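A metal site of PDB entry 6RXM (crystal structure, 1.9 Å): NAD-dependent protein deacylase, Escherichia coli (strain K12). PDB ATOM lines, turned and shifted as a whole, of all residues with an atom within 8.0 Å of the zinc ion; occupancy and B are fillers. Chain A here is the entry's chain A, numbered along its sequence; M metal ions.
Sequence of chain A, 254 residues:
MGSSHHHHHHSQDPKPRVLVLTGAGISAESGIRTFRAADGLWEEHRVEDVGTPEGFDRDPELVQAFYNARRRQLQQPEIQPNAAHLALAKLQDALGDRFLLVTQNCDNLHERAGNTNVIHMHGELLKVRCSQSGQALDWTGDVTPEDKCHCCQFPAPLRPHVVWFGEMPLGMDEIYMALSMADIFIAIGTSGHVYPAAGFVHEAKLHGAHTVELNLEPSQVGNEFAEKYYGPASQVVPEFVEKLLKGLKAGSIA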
ATOM      1  N   ARG A 129     -19.410 -18.375  -0.666  1.00  0.00           N
ATOM      2  CA  ARG A 129     -18.533 -19.111   0.232  1.00  0.00           C
ATOM      3  C   ARG A 129     -19.076 -19.089   1.654  1.00  0.00           C
ATOM      4  O   ARG A 129     -19.525 -18.051   2.127  1.00  0.00           O
ATOM      5  CB  ARG A 129     -17.131 -18.499   0.226  1.00  0.00           C
ATOM      6  CG  ARG A 129     -16.082 -19.279   0.988  1.00  0.00           C
ATOM      7  CD  ARG A 129     -14.825 -18.430   1.263  1.00  0.00           C
ATOM      8  NE  ARG A 129     -14.344 -17.789   0.049  1.00  0.00           N
ATOM      9  CZ  ARG A 129     -13.399 -16.853   0.022  1.00  0.00           C
ATOM     10  NH1 ARG A 129     -12.820 -16.454   1.145  1.00  0.00           N
ATOM     11  NH2 ARG A 129     -13.033 -16.314  -1.153  1.00  0.00           N
ATOM     12  N   CYS A 130     -19.008 -20.214   2.337  1.00  0.00           N
ATOM     13  CA  CYS A 130     -19.325 -20.225   3.762  1.00  0.00           C
ATOM     14  C   CYS A 130     -18.223 -19.510   4.514  1.00  0.00           C
ATOM     15  O   CYS A 130     -17.066 -19.937   4.484  1.00  0.00           O
ATOM     16  CB  CYS A 130     -19.471 -21.660   4.294  1.00  0.00           C
ATOM     17  SG  CYS A 130     -19.519 -21.635   6.094  1.00  0.00           S
ATOM     18  N   SER A 131     -18.595 -18.473   5.262  1.00  0.00           N
ATOM     19  CA  SER A 131     -17.634 -17.576   5.901  1.00  0.00           C
ATOM     20  C   SER A 131     -16.850 -18.222   7.048  1.00  0.00           C
ATOM     21  O   SER A 131     -15.946 -17.593   7.604  1.00  0.00           O
ATOM     22  CB  SER A 131     -18.378 -16.351   6.439  1.00  0.00           C
ATOM     23  OG  SER A 131     -19.377 -16.750   7.372  1.00  0.00           O
ATOM     24  N   GLN A 132     -17.206 -19.445   7.425  1.00  0.00           N
ATOM     25  CA  GLN A 132     -16.479 -20.177   8.460  1.00  0.00           C
ATOM     26  C   GLN A 132     -15.785 -21.423   7.877  1.00  0.00           C
ATOM     27  O   GLN A 132     -14.605 -21.691   8.173  1.00  0.00           O
ATOM     28  CB  GLN A 132     -17.406 -20.506   9.628  1.00  0.00           C
ATOM     29  CG  GLN A 132     -18.204 -21.766   9.543  1.00  0.00           C
ATOM     30  CD  GLN A 132     -18.875 -22.107  10.869  1.00  0.00           C
ATOM     31  OE1 GLN A 132     -18.509 -21.575  11.913  1.00  0.00           O
ATOM     32  NE2 GLN A 132     -19.824 -23.014  10.829  1.00  0.00           N
ATOM     33  N   SER A 133     -16.510 -22.186   7.072  1.00  0.00           N
ATOM     34  CA  SER A 133     -15.985 -23.373   6.416  1.00  0.00           C
ATOM     35  C   SER A 133     -15.048 -23.080   5.245  1.00  0.00           C
ATOM     36  O   SER A 133     -14.115 -23.826   4.984  1.00  0.00           O
ATOM     37  CB  SER A 133     -17.147 -24.233   5.919  1.00  0.00           C
ATOM     38  OG  SER A 133     -16.830 -24.852   4.701  1.00  0.00           O
ATOM     39  N   GLY A 134     -15.320 -21.997   4.537  1.00  0.00           N
ATOM     40  CA  GLY A 134     -14.556 -21.638   3.364  1.00  0.00           C
ATOM     41  C   GLY A 134     -14.991 -22.422   2.151  1.00  0.00           C
ATOM     42  O   GLY A 134     -14.452 -22.213   1.066  1.00  0.00           O
ATOM     43  N   GLN A 135     -15.980 -23.304   2.308  1.00  0.00           N
ATOM     44  CA  GLN A 135     -16.428 -24.078   1.145  1.00  0.00           C
ATOM     45  C   GLN A 135     -17.222 -23.179   0.236  1.00  0.00           C
ATOM     46  O   GLN A 135     -18.054 -22.397   0.699  1.00  0.00           O
ATOM     47  CB  GLN A 135     -17.269 -25.302   1.520  1.00  0.00           C
ATOM     48  CG  GLN A 135     -16.478 -26.485   2.046  1.00  0.00           C
ATOM     49  CD  GLN A 135     -17.398 -27.588   2.573  1.00  0.00           C
ATOM     50  OE1 GLN A 135     -18.496 -27.795   2.062  1.00  0.00           O
ATOM     51  NE2 GLN A 135     -16.906 -28.342   3.558  1.00  0.00           N
ATOM     52  N   LEU A 137     -19.723 -22.602  -3.284  1.00  0.00           N
ATOM     53  CA  LEU A 137     -20.738 -23.287  -4.062  1.00  0.00           C
ATOM     54  C   LEU A 137     -21.309 -22.378  -5.140  1.00  0.00           C
ATOM     55  O   LEU A 137     -21.318 -21.167  -5.001  1.00  0.00           O
ATOM     56  CB  LEU A 137     -21.816 -23.830  -3.133  1.00  0.00           C
ATOM     57  CG  LEU A 137     -22.528 -22.848  -2.213  1.00  0.00           C
ATOM     58  CD1 LEU A 137     -23.709 -22.199  -2.898  1.00  0.00           C
ATOM     59  CD2 LEU A 137     -22.956 -23.581  -0.943  1.00  0.00           C
ATOM     60  N   LYS A 148     -27.955 -19.157   4.116  1.00  0.00           N
ATOM     61  CA  LYS A 148     -26.869 -19.599   4.991  1.00  0.00           C
ATOM     62  C   LYS A 148     -26.310 -20.945   4.533  1.00  0.00           C
ATOM     63  O   LYS A 148     -26.917 -21.627   3.723  1.00  0.00           O
ATOM     64  CB  LYS A 148     -27.359 -19.654   6.441  1.00  0.00           C
ATOM     65  CG  LYS A 148     -27.454 -18.277   7.120  1.00  0.00           C
ATOM     66  CD  LYS A 148     -28.032 -18.359   8.511  1.00  0.00           C
ATOM     67  CE  LYS A 148     -28.087 -16.990   9.207  1.00  0.00           C
ATOM     68  NZ  LYS A 148     -29.011 -16.014   8.566  1.00  0.00           N
ATOM     69  N   CYS A 149     -25.142 -21.315   5.070  1.00  0.00           N
ATOM     70  CA  CYS A 149     -24.431 -22.503   4.583  1.00  0.00           C
ATOM     71  C   CYS A 149     -25.122 -23.803   4.987  1.00  0.00           C
ATOM     72  O   CYS A 149     -25.981 -23.820   5.858  1.00  0.00           O
ATOM     73  CB  CYS A 149     -23.004 -22.506   5.114  1.00  0.00           C
ATOM     74  SG  CYS A 149     -22.911 -23.022   6.849  1.00  0.00           S
ATOM     75  N   HIS A 150     -24.720 -24.880   4.315  1.00  0.00           N
ATOM     76  CA  HIS A 150     -25.218 -26.232   4.609  1.00  0.00           C
ATOM     77  C   HIS A 150     -24.061 -27.198   4.834  1.00  0.00           C
ATOM     78  O   HIS A 150     -24.206 -28.417   4.712  1.00  0.00           O
ATOM     79  CB  HIS A 150     -26.117 -26.748   3.493  1.00  0.00           C
ATOM     80  CG  HIS A 150     -27.282 -25.856   3.195  1.00  0.00           C
ATOM     81  ND1 HIS A 150     -28.314 -25.656   4.090  1.00  0.00           N
ATOM     82  CD2 HIS A 150     -27.589 -25.124   2.110  1.00  0.00           C
ATOM     83  CE1 HIS A 150     -29.200 -24.833   3.572  1.00  0.00           C
ATOM     84  NE2 HIS A 150     -28.785 -24.486   2.362  1.00  0.00           N
ATOM     85  N   CYS A 151     -22.896 -26.636   5.154  1.00  0.00           N
ATOM     86  CA  CYS A 151     -21.654 -27.389   5.262  1.00  0.00           C
ATOM     87  C   CYS A 151     -21.268 -27.448   6.722  1.00  0.00           C
ATOM     88  O   CYS A 151     -20.286 -28.105   7.099  1.00  0.00           O
ATOM     89  CB  CYS A 151     -20.545 -26.692   4.463  1.00  0.00           C
ATOM     90  SG  CYS A 151     -20.391 -24.890   4.837  1.00  0.00           S
ATOM     91  N   CYS A 152     -22.036 -26.745   7.537  1.00  0.00           N
ATOM     92  CA  CYS A 152     -21.753 -26.627   8.980  1.00  0.00           C
ATOM     93  C   CYS A 152     -22.816 -27.015  10.022  1.00  0.00           C
ATOM     94  O   CYS A 152     -24.011 -27.163   9.754  1.00  0.00           O
ATOM     95  CB  CYS A 152     -21.292 -25.211   9.240  1.00  0.00           C
ATOM     96  SG  CYS A 152     -19.798 -24.784   8.360  1.00  0.00           S
ATOM     97  N   GLN A 153     -22.321 -27.174  11.245  1.00  0.00           N
ATOM     98  CA  GLN A 153     -23.165 -27.583  12.352  1.00  0.00           C
ATOM     99  C   GLN A 153     -24.229 -26.511  12.657  1.00  0.00           C
ATOM    100  O   GLN A 153     -25.409 -26.820  12.782  1.00  0.00           O
ATOM    101  CB  GLN A 153     -22.296 -27.810  13.598  1.00  0.00           C
ATOM    102  CG  GLN A 153     -23.067 -28.305  14.783  1.00  0.00           C
ATOM    103  CD  GLN A 153     -23.662 -29.660  14.453  1.00  0.00           C
ATOM    104  OE1 GLN A 153     -22.950 -30.579  14.071  1.00  0.00           O
ATOM    105  NE2 GLN A 153     -24.980 -29.769  14.576  1.00  0.00           N
ATOM    106  N   PHE A 154     -23.805 -25.255  12.721  1.00  0.00           N
ATOM    107  CA  PHE A 154     -24.739 -24.124  12.811  1.00  0.00           C
ATOM    108  C   PHE A 154     -24.591 -23.235  11.592  1.00  0.00           C
ATOM    109  O   PHE A 154     -23.615 -22.489  11.513  1.00  0.00           O
ATOM    110  CB  PHE A 154     -24.522 -23.304  14.071  1.00  0.00           C
ATOM    111  CG  PHE A 154     -24.758 -24.068  15.334  1.00  0.00           C
ATOM    112  CD1 PHE A 154     -25.522 -25.220  15.334  1.00  0.00           C
ATOM    113  CD2 PHE A 154     -24.220 -23.623  16.518  1.00  0.00           C
ATOM    114  CE1 PHE A 154     -25.736 -25.926  16.489  1.00  0.00           C
ATOM    115  CE2 PHE A 154     -24.437 -24.323  17.665  1.00  0.00           C
ATOM    116  CZ  PHE A 154     -25.190 -25.467  17.666  1.00  0.00           C
ATOM    117  N   PRO A 155     -25.575 -23.262  10.688  1.00  0.00           N
ATOM    118  CA  PRO A 155     -25.493 -22.583   9.389  1.00  0.00           C
ATOM    119  C   PRO A 155     -25.023 -21.138   9.538  1.00  0.00           C
ATOM    120  O   PRO A 155     -25.550 -20.380  10.360  1.00  0.00           O
ATOM    121  CB  PRO A 155     -26.920 -22.651   8.860  1.00  0.00           C
ATOM    122  CG  PRO A 155     -27.532 -23.822   9.537  1.00  0.00           C
ATOM    123  CD  PRO A 155     -26.863 -23.958  10.872  1.00  0.00           C
ATOM    124  N   ALA A 156     -23.991 -20.796   8.769  1.00  0.00           N
ATOM    125  CA  ALA A 156     -23.321 -19.494   8.856  1.00  0.00           C
ATOM    126  C   ALA A 156     -23.641 -18.630   7.650  1.00  0.00           C
ATOM    127  O   ALA A 156     -23.984 -19.145   6.609  1.00  0.00           O
ATOM    128  CB  ALA A 156     -21.809 -19.708   8.984  1.00  0.00           C
ATOM    129  N   PRO A 157     -23.497 -17.305   7.794  1.00  0.00           N
ATOM    130  CA  PRO A 157     -23.718 -16.386   6.675  1.00  0.00           C
ATOM    131  C   PRO A 157     -22.809 -16.709   5.478  1.00  0.00           C
ATOM    132  O   PRO A 157     -21.696 -17.216   5.663  1.00  0.00           O
ATOM    133  CB  PRO A 157     -23.353 -15.021   7.267  1.00  0.00           C
ATOM    134  CG  PRO A 157     -23.537 -15.181   8.730  1.00  0.00           C
ATOM    135  CD  PRO A 157     -23.149 -16.587   9.034  1.00  0.00           C
ATOM    136  N   LEU A 158     -23.296 -16.444   4.273  1.00  0.00           N
ATOM    137  CA  LEU A 158     -22.534 -16.697   3.054  1.00  0.00           C
ATOM    138  C   LEU A 158     -21.963 -15.382   2.593  1.00  0.00           C
ATOM    139  O   LEU A 158     -22.605 -14.353   2.716  1.00  0.00           O
ATOM    140  CB  LEU A 158     -23.424 -17.300   1.964  1.00  0.00           C
ATOM    141  CG  LEU A 158     -23.989 -18.677   2.306  1.00  0.00           C
ATOM    142  CD1 LEU A 158     -25.067 -19.101   1.309  1.00  0.00           C
ATOM    143  CD2 LEU A 158     -22.871 -19.716   2.408  1.00  0.00           C
HETATM  144 ZN    ZN M   1     -20.663 -23.578   6.672  1.00  0.00          ZN
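The backbone NH (N) of Cys 130 sits at hydrogen-bond distance from the backbone carbonyl oxygen (O) of Gln 135 (2.9 Å). SG of Cys 130 lies close to N of Gln 132, at 3.5 Å. The side-chain hydroxyl of Ser 133 lies within hydrogen-bond range of the backbone NH of Gln 135 (3.0 Å). SG of Cys 152 sits close to NE2 of Gln 132, 3.0 Å away. The side-chain sulfur (SG) of Cys 130 sits close to the backbone NH (N) of Ser 133. The backbone NH (N) of Cys 149 is in hydrogen-bond range of the backbone carbonyl oxygen (O) of Ala 156 (2.9 Å). The side-chain hydroxyl (OG) of Ser 133 sits close to the side-chain sulfur (SG) of Cys 151.
Ser 133 touches the zinc ion. Five residues have an atom within 4 Å of the zinc ion: Cys 130, Ser 133, Cys 149, Cys 151 and Cys 152.
The zinc ion is bound by the side-chain sulfur (SG) of Cys 152 (2.2 Å), the side-chain sulfur (SG) of Cys 151 (2.3 Å), the side-chain sulfur (SG) of Cys 149 (2.3 Å) and the side-chain sulfur (SG) of Cys 130 (2.3 Å). The zinc ion has four donor atoms within binding distance.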
